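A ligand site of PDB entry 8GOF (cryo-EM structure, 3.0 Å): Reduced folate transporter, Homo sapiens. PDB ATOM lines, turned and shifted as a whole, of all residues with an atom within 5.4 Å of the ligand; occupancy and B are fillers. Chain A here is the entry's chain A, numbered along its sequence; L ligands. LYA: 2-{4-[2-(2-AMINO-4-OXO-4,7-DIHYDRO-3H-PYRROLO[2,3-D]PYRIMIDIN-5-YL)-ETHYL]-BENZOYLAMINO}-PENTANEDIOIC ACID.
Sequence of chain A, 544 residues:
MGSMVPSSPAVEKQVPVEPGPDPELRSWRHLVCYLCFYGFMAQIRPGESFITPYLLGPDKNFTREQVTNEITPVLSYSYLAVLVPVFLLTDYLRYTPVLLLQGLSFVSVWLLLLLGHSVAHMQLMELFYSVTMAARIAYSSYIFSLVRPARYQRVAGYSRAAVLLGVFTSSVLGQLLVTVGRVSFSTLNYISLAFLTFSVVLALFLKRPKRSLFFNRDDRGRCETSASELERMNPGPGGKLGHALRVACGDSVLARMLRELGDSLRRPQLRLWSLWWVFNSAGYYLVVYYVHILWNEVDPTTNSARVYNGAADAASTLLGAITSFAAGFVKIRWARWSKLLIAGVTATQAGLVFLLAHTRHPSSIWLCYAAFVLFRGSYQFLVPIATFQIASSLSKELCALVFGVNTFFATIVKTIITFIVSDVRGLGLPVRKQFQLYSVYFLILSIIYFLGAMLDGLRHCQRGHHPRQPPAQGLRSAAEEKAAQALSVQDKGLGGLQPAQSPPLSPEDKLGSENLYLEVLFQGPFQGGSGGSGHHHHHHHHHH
Ile 51 touches the ligand (CG2 to N18, 3.7 Å).
CD1 of Leu 55 touches N19 of the ligand (3.4 Å).
Val 67 touches the ligand.
Leu 75 touches the ligand (CD2 to C7, 3.4 Å).
Met 125 touches the ligand.
Tyr 129 touches the ligand.
SD of Met 133 touches C2 of the ligand (3.6 Å).
Val 167 touches the ligand.
CE1 of Tyr 285 touches O21 of the ligand (3.1 Å).
Val 288 touches the ligand (CG1 to C5, 3.8 Å).
CE1 of Tyr 289 touches C2 of the ligand (3.1 Å).
Gln 380 touches the ligand (NE2 to O30, 3.8 Å).
18 residues have an atom within 4 Å of the ligand: Ile 51, Thr 52, Leu 55, Val 67, Leu 75, Met 125, Glu 126, Tyr 129, Met 133, Arg 136, Val 167, Tyr 284, Tyr 285, Val 288, Tyr 289, Thr 317, Arg 376 and Gln 380.
Along chain A the residues within 4 Å of the ligand span positions 51 to 380.
The guanidinium group (NE) of Arg 376 is in hydrogen-bond range of the side-chain hydroxyl (OH) of Tyr 284 (3.2 Å).
The guanidinium group of Arg 376 is in salt-bridge range of the side-chain carboxylate of Asp 313, 3.997 Å away.
The side-chain hydroxyl (OH) of Tyr 129 lies within hydrogen-bond range of the side-chain carboxylate (OE2) of Glu 48.
The side-chain hydroxyl (OG1) of Thr 317 is in hydrogen-bond range of the backbone carbonyl oxygen (O) of Asp 313, at 2.7 Å.
OG of Ser 171 lies within hydrogen-bond range of O of Val 167.
The backbone carbonyl oxygen of Val 67 is in hydrogen-bond range of the backbone NH of Thr 72, at 2.9 Å.
The side-chain hydroxyl of Thr 52 is in hydrogen-bond range of a nitrogen (N16) of the ligand.
N11 of the ligand lies within hydrogen-bond range of OE1 of Glu 126 (3.0 Å).
The guanidinium group (NH1) of Arg 136 is in hydrogen-bond range of an oxygen (O21) of the ligand (2.8 Å).
The guanidinium group of Arg 376 is in salt-bridge range of an oxygen (O31) of the ligand (2.8 Å).
An oxygen (O31) of the ligand is in hydrogen-bond range of the side-chain hydroxyl (OH) of Tyr 284, at 3.0 Å.
OG1 of Thr 317 is in hydrogen-bond range of O27 of the ligand (3.3 Å).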
ATOM      1  N   GLU A  48      14.935  -0.612   8.536  1.00  0.00           N
ATOM      2  CA  GLU A  48      16.225  -1.131   8.100  1.00  0.00           C
ATOM      3  C   GLU A  48      16.129  -1.803   6.744  1.00  0.00           C
ATOM      4  O   GLU A  48      17.009  -1.629   5.894  1.00  0.00           O
ATOM      5  CB  GLU A  48      16.770  -2.108   9.142  1.00  0.00           C
ATOM      6  CG  GLU A  48      18.076  -2.761   8.757  1.00  0.00           C
ATOM      7  CD  GLU A  48      18.659  -3.567   9.886  1.00  0.00           C
ATOM      8  OE1 GLU A  48      18.732  -3.038  11.008  1.00  0.00           O
ATOM      9  OE2 GLU A  48      19.055  -4.727   9.636  1.00  0.00           O
ATOM     10  N   ILE A  51      15.930   0.935   3.743  1.00  0.00           N
ATOM     11  CA  ILE A  51      16.947   1.970   3.614  1.00  0.00           C
ATOM     12  C   ILE A  51      17.158   2.316   2.145  1.00  0.00           C
ATOM     13  O   ILE A  51      17.129   3.482   1.761  1.00  0.00           O
ATOM     14  CB  ILE A  51      18.264   1.534   4.294  1.00  0.00           C
ATOM     15  CG1 ILE A  51      18.106   1.557   5.810  1.00  0.00           C
ATOM     16  CG2 ILE A  51      19.417   2.421   3.877  1.00  0.00           C
ATOM     17  CD1 ILE A  51      19.325   1.096   6.555  1.00  0.00           C
ATOM     18  N   THR A  52      17.343   1.302   1.313  1.00  0.00           N
ATOM     19  CA  THR A  52      17.522   1.465  -0.123  1.00  0.00           C
ATOM     20  C   THR A  52      16.288   2.012  -0.847  1.00  0.00           C
ATOM     21  O   THR A  52      16.458   2.940  -1.652  1.00  0.00           O
ATOM     22  CB  THR A  52      17.996   0.139  -0.742  1.00  0.00           C
ATOM     23  OG1 THR A  52      19.320  -0.150  -0.308  1.00  0.00           O
ATOM     24  CG2 THR A  52      17.983   0.197  -2.250  1.00  0.00           C
ATOM     25  N   LEU A  55      16.508   5.687   0.142  1.00  0.00           N
ATOM     26  CA  LEU A  55      17.594   6.431  -0.496  1.00  0.00           C
ATOM     27  C   LEU A  55      17.346   6.623  -1.987  1.00  0.00           C
ATOM     28  O   LEU A  55      17.719   7.654  -2.546  1.00  0.00           O
ATOM     29  CB  LEU A  55      18.929   5.724  -0.300  1.00  0.00           C
ATOM     30  CG  LEU A  55      19.559   5.644   1.091  1.00  0.00           C
ATOM     31  CD1 LEU A  55      20.880   4.930   1.000  1.00  0.00           C
ATOM     32  CD2 LEU A  55      19.726   7.022   1.689  1.00  0.00           C
ATOM     33  N   VAL A  67      23.956   5.161  -5.536  1.00  0.00           N
ATOM     34  CA  VAL A  67      23.775   4.287  -4.394  1.00  0.00           C
ATOM     35  C   VAL A  67      24.511   2.968  -4.609  1.00  0.00           C
ATOM     36  O   VAL A  67      25.225   2.489  -3.718  1.00  0.00           O
ATOM     37  CB  VAL A  67      22.281   4.080  -4.128  1.00  0.00           C
ATOM     38  CG1 VAL A  67      22.049   2.992  -3.099  1.00  0.00           C
ATOM     39  CG2 VAL A  67      21.670   5.378  -3.647  1.00  0.00           C
ATOM     40  N   ILE A  71      27.910   4.539  -2.732  1.00  0.00           N
ATOM     41  CA  ILE A  71      27.468   4.428  -1.346  1.00  0.00           C
ATOM     42  C   ILE A  71      27.604   3.008  -0.824  1.00  0.00           C
ATOM     43  O   ILE A  71      28.265   2.773   0.186  1.00  0.00           O
ATOM     44  CB  ILE A  71      26.016   4.939  -1.194  1.00  0.00           C
ATOM     45  CG1 ILE A  71      25.949   6.439  -1.433  1.00  0.00           C
ATOM     46  CG2 ILE A  71      25.488   4.630   0.177  1.00  0.00           C
ATOM     47  CD1 ILE A  71      24.542   6.938  -1.625  1.00  0.00           C
ATOM     48  N   THR A  72      26.985   2.048  -1.497  1.00  0.00           N
ATOM     49  CA  THR A  72      26.967   0.651  -1.046  1.00  0.00           C
ATOM     50  C   THR A  72      28.334  -0.054  -1.012  1.00  0.00           C
ATOM     51  O   THR A  72      28.504  -0.938  -0.168  1.00  0.00           O
ATOM     52  CB  THR A  72      25.979  -0.153  -1.902  1.00  0.00           C
ATOM     53  OG1 THR A  72      24.875   0.697  -2.249  1.00  0.00           O
ATOM     54  CG2 THR A  72      25.431  -1.334  -1.139  1.00  0.00           C
ATOM     55  N   LEU A  75      29.887   0.159   2.462  1.00  0.00           N
ATOM     56  CA  LEU A  75      29.450  -0.819   3.437  1.00  0.00           C
ATOM     57  C   LEU A  75      30.423  -1.986   3.566  1.00  0.00           C
ATOM     58  O   LEU A  75      30.476  -2.614   4.624  1.00  0.00           O
ATOM     59  CB  LEU A  75      28.067  -1.346   3.071  1.00  0.00           C
ATOM     60  CG  LEU A  75      27.272  -2.174   4.072  1.00  0.00           C
ATOM     61  CD1 LEU A  75      27.308  -1.524   5.434  1.00  0.00           C
ATOM     62  CD2 LEU A  75      25.848  -2.309   3.587  1.00  0.00           C
ATOM     63  N   MET A 125      27.290   7.119   6.599  1.00  0.00           N
ATOM     64  CA  MET A 125      26.270   6.227   7.131  1.00  0.00           C
ATOM     65  C   MET A 125      26.661   4.769   6.966  1.00  0.00           C
ATOM     66  O   MET A 125      26.323   3.941   7.819  1.00  0.00           O
ATOM     67  CB  MET A 125      24.934   6.497   6.436  1.00  0.00           C
ATOM     68  CG  MET A 125      23.756   5.792   7.034  1.00  0.00           C
ATOM     69  SD  MET A 125      22.399   5.694   5.867  1.00  0.00           S
ATOM     70  CE  MET A 125      22.936   4.331   4.840  1.00  0.00           C
ATOM     71  N   GLU A 126      27.379   4.426   5.900  1.00  0.00           N
ATOM     72  CA  GLU A 126      27.911   3.082   5.764  1.00  0.00           C
ATOM     73  C   GLU A 126      29.112   2.835   6.664  1.00  0.00           C
ATOM     74  O   GLU A 126      29.419   1.682   6.953  1.00  0.00           O
ATOM     75  CB  GLU A 126      28.313   2.791   4.322  1.00  0.00           C
ATOM     76  CG  GLU A 126      27.269   3.148   3.289  1.00  0.00           C
ATOM     77  CD  GLU A 126      26.040   2.264   3.346  1.00  0.00           C
ATOM     78  OE1 GLU A 126      26.103   1.141   3.865  1.00  0.00           O
ATOM     79  OE2 GLU A 126      24.983   2.707   2.832  1.00  0.00           O
ATOM     80  N   TYR A 129      27.191   2.016   9.836  1.00  0.00           N
ATOM     81  CA  TYR A 129      26.480   0.748   9.754  1.00  0.00           C
ATOM     82  C   TYR A 129      27.440  -0.433   9.847  1.00  0.00           C
ATOM     83  O   TYR A 129      27.069  -1.481  10.374  1.00  0.00           O
ATOM     84  CB  TYR A 129      25.671   0.664   8.465  1.00  0.00           C
ATOM     85  CG  TYR A 129      24.549  -0.345   8.541  1.00  0.00           C
ATOM     86  CD1 TYR A 129      24.759  -1.675   8.209  1.00  0.00           C
ATOM     87  CD2 TYR A 129      23.284   0.045   8.950  1.00  0.00           C
ATOM     88  CE1 TYR A 129      23.744  -2.592   8.292  1.00  0.00           C
ATOM     89  CE2 TYR A 129      22.256  -0.869   9.028  1.00  0.00           C
ATOM     90  CZ  TYR A 129      22.499  -2.187   8.698  1.00  0.00           C
ATOM     91  OH  TYR A 129      21.490  -3.103   8.765  1.00  0.00           O
ATOM     92  N   MET A 133      27.747  -3.891  12.242  1.00  0.00           N
ATOM     93  CA  MET A 133      27.868  -5.273  11.714  1.00  0.00           C
ATOM     94  C   MET A 133      29.083  -5.944  12.364  1.00  0.00           C
ATOM     95  O   MET A 133      29.021  -7.159  12.601  1.00  0.00           O
ATOM     96  CB  MET A 133      28.001  -5.275  10.196  1.00  0.00           C
ATOM     97  CG  MET A 133      26.724  -4.863   9.499  1.00  0.00           C
ATOM     98  SD  MET A 133      27.074  -4.298   7.817  1.00  0.00           S
ATOM     99  CE  MET A 133      28.486  -5.326   7.448  1.00  0.00           C
ATOM    100  N   ARG A 136      28.206  -7.136  15.920  1.00  0.00           N
ATOM    101  CA  ARG A 136      27.094  -8.073  16.006  1.00  0.00           C
ATOM    102  C   ARG A 136      27.454  -9.262  16.881  1.00  0.00           C
ATOM    103  O   ARG A 136      26.575  -9.864  17.513  1.00  0.00           O
ATOM    104  CB  ARG A 136      26.678  -8.525  14.610  1.00  0.00           C
ATOM    105  CG  ARG A 136      25.278  -9.058  14.505  1.00  0.00           C
ATOM    106  CD  ARG A 136      24.802  -8.924  13.080  1.00  0.00           C
ATOM    107  NE  ARG A 136      25.830  -9.356  12.142  1.00  0.00           N
ATOM    108  CZ  ARG A 136      25.878  -8.991  10.871  1.00  0.00           C
ATOM    109  NH1 ARG A 136      24.956  -8.165  10.377  1.00  0.00           N
ATOM    110  NH2 ARG A 136      26.853  -9.434  10.087  1.00  0.00           N
ATOM    111  N   VAL A 167      14.717  -9.642  15.130  1.00  0.00           N
ATOM    112  CA  VAL A 167      14.892  -9.337  13.718  1.00  0.00           C
ATOM    113  C   VAL A 167      13.713  -9.809  12.883  1.00  0.00           C
ATOM    114  O   VAL A 167      13.541  -9.350  11.751  1.00  0.00           O
ATOM    115  CB  VAL A 167      16.180  -9.969  13.147  1.00  0.00           C
ATOM    116  CG1 VAL A 167      17.390  -9.261  13.697  1.00  0.00           C
ATOM    117  CG2 VAL A 167      16.240 -11.428  13.486  1.00  0.00           C
ATOM    118  N   SER A 171      11.103  -6.489  11.054  1.00  0.00           N
ATOM    119  CA  SER A 171      10.720  -6.462   9.651  1.00  0.00           C
ATOM    120  C   SER A 171       9.209  -6.633   9.477  1.00  0.00           C
ATOM    121  O   SER A 171       8.672  -6.187   8.467  1.00  0.00           O
ATOM    122  CB  SER A 171      11.476  -7.549   8.897  1.00  0.00           C
ATOM    123  OG  SER A 171      12.867  -7.344   9.002  1.00  0.00           O
ATOM    124  N   TYR A 284      27.682 -14.030  -0.341  1.00  0.00           N
ATOM    125  CA  TYR A 284      26.336 -13.976   0.231  1.00  0.00           C
ATOM    126  C   TYR A 284      25.976 -12.547   0.624  1.00  0.00           C
ATOM    127  O   TYR A 284      24.875 -12.077   0.320  1.00  0.00           O
ATOM    128  CB  TYR A 284      26.243 -14.897   1.442  1.00  0.00           C
ATOM    129  CG  TYR A 284      25.036 -14.639   2.318  1.00  0.00           C
ATOM    130  CD1 TYR A 284      23.777 -15.069   1.935  1.00  0.00           C
ATOM    131  CD2 TYR A 284      25.155 -13.996   3.538  1.00  0.00           C
ATOM    132  CE1 TYR A 284      22.681 -14.851   2.721  1.00  0.00           C
ATOM    133  CE2 TYR A 284      24.056 -13.771   4.336  1.00  0.00           C
ATOM    134  CZ  TYR A 284      22.823 -14.201   3.926  1.00  0.00           C
ATOM    135  OH  TYR A 284      21.732 -13.980   4.720  1.00  0.00           O
ATOM    136  N   TYR A 285      26.877 -11.853   1.312  1.00  0.00           N
ATOM    137  CA  TYR A 285      26.585 -10.495   1.732  1.00  0.00           C
ATOM    138  C   TYR A 285      26.610  -9.513   0.568  1.00  0.00           C
ATOM    139  O   TYR A 285      25.968  -8.468   0.659  1.00  0.00           O
ATOM    140  CB  TYR A 285      27.556 -10.060   2.830  1.00  0.00           C
ATOM    141  CG  TYR A 285      27.328 -10.792   4.128  1.00  0.00           C
ATOM    142  CD1 TYR A 285      26.139 -10.659   4.813  1.00  0.00           C
ATOM    143  CD2 TYR A 285      28.312 -11.607   4.667  1.00  0.00           C
ATOM    144  CE1 TYR A 285      25.925 -11.331   6.004  1.00  0.00           C
ATOM    145  CE2 TYR A 285      28.109 -12.276   5.850  1.00  0.00           C
ATOM    146  CZ  TYR A 285      26.913 -12.139   6.514  1.00  0.00           C
ATOM    147  OH  TYR A 285      26.724 -12.810   7.701  1.00  0.00           O
ATOM    148  N   VAL A 288      23.222  -9.754  -0.428  1.00  0.00           N
ATOM    149  CA  VAL A 288      22.377  -9.180   0.626  1.00  0.00           C
ATOM    150  C   VAL A 288      22.421  -7.658   0.589  1.00  0.00           C
ATOM    151  O   VAL A 288      21.390  -6.985   0.749  1.00  0.00           O
ATOM    152  CB  VAL A 288      22.806  -9.766   1.987  1.00  0.00           C
ATOM    153  CG1 VAL A 288      22.345  -8.909   3.143  1.00  0.00           C
ATOM    154  CG2 VAL A 288      22.245 -11.154   2.135  1.00  0.00           C
ATOM    155  N   TYR A 289      23.598  -7.076   0.336  1.00  0.00           N
ATOM    156  CA  TYR A 289      23.722  -5.617   0.282  1.00  0.00           C
ATOM    157  C   TYR A 289      22.998  -5.024  -0.909  1.00  0.00           C
ATOM    158  O   TYR A 289      22.466  -3.909  -0.830  1.00  0.00           O
ATOM    159  CB  TYR A 289      25.185  -5.184   0.210  1.00  0.00           C
ATOM    160  CG  TYR A 289      26.068  -5.523   1.393  1.00  0.00           C
ATOM    161  CD1 TYR A 289      25.526  -5.845   2.632  1.00  0.00           C
ATOM    162  CD2 TYR A 289      27.446  -5.518   1.250  1.00  0.00           C
ATOM    163  CE1 TYR A 289      26.345  -6.162   3.692  1.00  0.00           C
ATOM    164  CE2 TYR A 289      28.269  -5.826   2.305  1.00  0.00           C
ATOM    165  CZ  TYR A 289      27.716  -6.153   3.528  1.00  0.00           C
ATOM    166  OH  TYR A 289      28.542  -6.453   4.579  1.00  0.00           O
ATOM    167  N   HIS A 292      18.255  -5.077  -2.590  1.00  0.00           N
ATOM    168  CA  HIS A 292      17.207  -4.073  -2.464  1.00  0.00           C
ATOM    169  C   HIS A 292      17.332  -3.004  -3.544  1.00  0.00           C
ATOM    170  O   HIS A 292      16.333  -2.372  -3.892  1.00  0.00           O
ATOM    171  CB  HIS A 292      17.268  -3.442  -1.076  1.00  0.00           C
ATOM    172  CG  HIS A 292      16.808  -4.338   0.022  1.00  0.00           C
ATOM    173  ND1 HIS A 292      16.681  -3.923   1.329  1.00  0.00           N
ATOM    174  CD2 HIS A 292      16.431  -5.637   0.014  1.00  0.00           C
ATOM    175  CE1 HIS A 292      16.257  -4.924   2.077  1.00  0.00           C
ATOM    176  NE2 HIS A 292      16.092  -5.981   1.295  1.00  0.00           N
ATOM    177  N   ASP A 313      12.308  -9.693   4.290  1.00  0.00           N
ATOM    178  CA  ASP A 313      13.342  -9.837   5.294  1.00  0.00           C
ATOM    179  C   ASP A 313      12.811 -10.415   6.597  1.00  0.00           C
ATOM    180  O   ASP A 313      13.599 -10.677   7.505  1.00  0.00           O
ATOM    181  CB  ASP A 313      14.021  -8.487   5.564  1.00  0.00           C
ATOM    182  CG  ASP A 313      14.910  -8.048   4.423  1.00  0.00           C
ATOM    183  OD1 ASP A 313      14.977  -8.769   3.401  1.00  0.00           O
ATOM    184  OD2 ASP A 313      15.553  -6.984   4.541  1.00  0.00           O
ATOM    185  N   THR A 317      14.089 -14.345   7.480  1.00  0.00           N
ATOM    186  CA  THR A 317      14.429 -14.607   8.877  1.00  0.00           C
ATOM    187  C   THR A 317      13.718 -15.849   9.371  1.00  0.00           C
ATOM    188  O   THR A 317      14.324 -16.695  10.056  1.00  0.00           O
ATOM    189  CB  THR A 317      14.076 -13.389   9.728  1.00  0.00           C
ATOM    190  OG1 THR A 317      14.864 -12.266   9.317  1.00  0.00           O
ATOM    191  CG2 THR A 317      14.325 -13.665  11.194  1.00  0.00           C
ATOM    192  N   ARG A 376      18.569 -16.764   1.272  1.00  0.00           N
ATOM    193  CA  ARG A 376      18.992 -16.581   2.654  1.00  0.00           C
ATOM    194  C   ARG A 376      18.847 -17.903   3.397  1.00  0.00           C
ATOM    195  O   ARG A 376      19.685 -18.241   4.237  1.00  0.00           O
ATOM    196  CB  ARG A 376      18.163 -15.487   3.342  1.00  0.00           C
ATOM    197  CG  ARG A 376      18.480 -14.080   2.855  1.00  0.00           C
ATOM    198  CD  ARG A 376      17.974 -13.031   3.842  1.00  0.00           C
ATOM    199  NE  ARG A 376      19.062 -12.225   4.377  1.00  0.00           N
ATOM    200  CZ  ARG A 376      18.884 -11.173   5.171  1.00  0.00           C
ATOM    201  NH1 ARG A 376      17.669 -10.812   5.536  1.00  0.00           N
ATOM    202  NH2 ARG A 376      19.936 -10.490   5.619  1.00  0.00           N
ATOM    203  N   TYR A 379      21.733 -20.229   2.685  1.00  0.00           N
ATOM    204  CA  TYR A 379      22.957 -19.898   3.413  1.00  0.00           C
ATOM    205  C   TYR A 379      22.809 -20.167   4.895  1.00  0.00           C
ATOM    206  O   TYR A 379      23.758 -20.634   5.538  1.00  0.00           O
ATOM    207  CB  TYR A 379      23.322 -18.436   3.169  1.00  0.00           C
ATOM    208  CG  TYR A 379      24.488 -17.924   3.977  1.00  0.00           C
ATOM    209  CD1 TYR A 379      25.790 -18.165   3.589  1.00  0.00           C
ATOM    210  CD2 TYR A 379      24.276 -17.159   5.119  1.00  0.00           C
ATOM    211  CE1 TYR A 379      26.850 -17.690   4.314  1.00  0.00           C
ATOM    212  CE2 TYR A 379      25.330 -16.685   5.860  1.00  0.00           C
ATOM    213  CZ  TYR A 379      26.618 -16.954   5.452  1.00  0.00           C
ATOM    214  OH  TYR A 379      27.667 -16.467   6.193  1.00  0.00           O
ATOM    215  N   GLN A 380      21.637 -19.899   5.462  1.00  0.00           N
ATOM    216  CA  GLN A 380      21.412 -20.170   6.883  1.00  0.00           C
ATOM    217  C   GLN A 380      21.230 -21.652   7.179  1.00  0.00           C
ATOM    218  O   GLN A 380      21.105 -22.013   8.352  1.00  0.00           O
ATOM    219  CB  GLN A 380      20.204 -19.398   7.392  1.00  0.00           C
ATOM    220  CG  GLN A 380      20.435 -17.902   7.539  1.00  0.00           C
ATOM    221  CD  GLN A 380      21.371 -17.576   8.676  1.00  0.00           C
ATOM    222  OE1 GLN A 380      21.317 -18.182   9.743  1.00  0.00           O
ATOM    223  NE2 GLN A 380      22.257 -16.610   8.453  1.00  0.00           N
HETATM  224  C1  LYA L   1      23.136  -5.103   5.642  1.00  0.00           C
HETATM  225  C2  LYA L   1      24.335  -5.677   6.001  1.00  0.00           C
HETATM  226  C3  LYA L   1      24.405  -6.913   6.607  1.00  0.00           C
HETATM  227  C4  LYA L   1      23.242  -7.633   6.854  1.00  0.00           C
HETATM  228  C5  LYA L   1      22.027  -7.081   6.487  1.00  0.00           C
HETATM  229  C6  LYA L   1      21.984  -5.835   5.874  1.00  0.00           C
HETATM  230  C7  LYA L   1      23.080  -3.777   4.944  1.00  0.00           C
HETATM  231  C8  LYA L   1      21.901  -2.856   5.253  1.00  0.00           C
HETATM  232  C9  LYA L   1      22.340  -1.479   4.894  1.00  0.00           C
HETATM  233  C10 LYA L   1      23.103  -0.636   5.657  1.00  0.00           C
HETATM  234  N11 LYA L   1      23.350   0.516   4.984  1.00  0.00           N
HETATM  235  C12 LYA L   1      22.776   0.408   3.754  1.00  0.00           C
HETATM  236  C13 LYA L   1      22.137  -0.804   3.650  1.00  0.00           C
HETATM  237  C14 LYA L   1      21.444  -1.128   2.441  1.00  0.00           C
HETATM  238  O15 LYA L   1      20.849  -2.200   2.273  1.00  0.00           O
HETATM  239  N16 LYA L   1      21.405  -0.238   1.400  1.00  0.00           N
HETATM  240  C17 LYA L   1      22.042   0.923   1.543  1.00  0.00           C
HETATM  241  N18 LYA L   1      22.694   1.266   2.687  1.00  0.00           N
HETATM  242  N19 LYA L   1      22.027   1.809   0.536  1.00  0.00           N
HETATM  243  C20 LYA L   1      23.358  -8.969   7.532  1.00  0.00           C
HETATM  244  O21 LYA L   1      24.453  -9.383   7.919  1.00  0.00           O
HETATM  245  N22 LYA L   1      22.232  -9.664   7.715  1.00  0.00           N
HETATM  246  C23 LYA L   1      22.151 -10.722   8.706  1.00  0.00           C
HETATM  247  C24 LYA L   1      20.955 -10.522   9.663  1.00  0.00           C
HETATM  248  C25 LYA L   1      19.717  -9.998   8.960  1.00  0.00           C
HETATM  249  C26 LYA L   1      18.404 -10.489   9.554  1.00  0.00           C
HETATM  250  O27 LYA L   1      17.338 -10.072   9.053  1.00  0.00           O
HETATM  251  O28 LYA L   1      18.455 -11.282  10.515  1.00  0.00           O
HETATM  252  C29 LYA L   1      22.172 -12.117   8.050  1.00  0.00           C
HETATM  253  O30 LYA L   1      23.112 -12.870   8.371  1.00  0.00           O
HETATM  254  O31 LYA L   1      21.271 -12.395   7.249  1.00  0.00           O
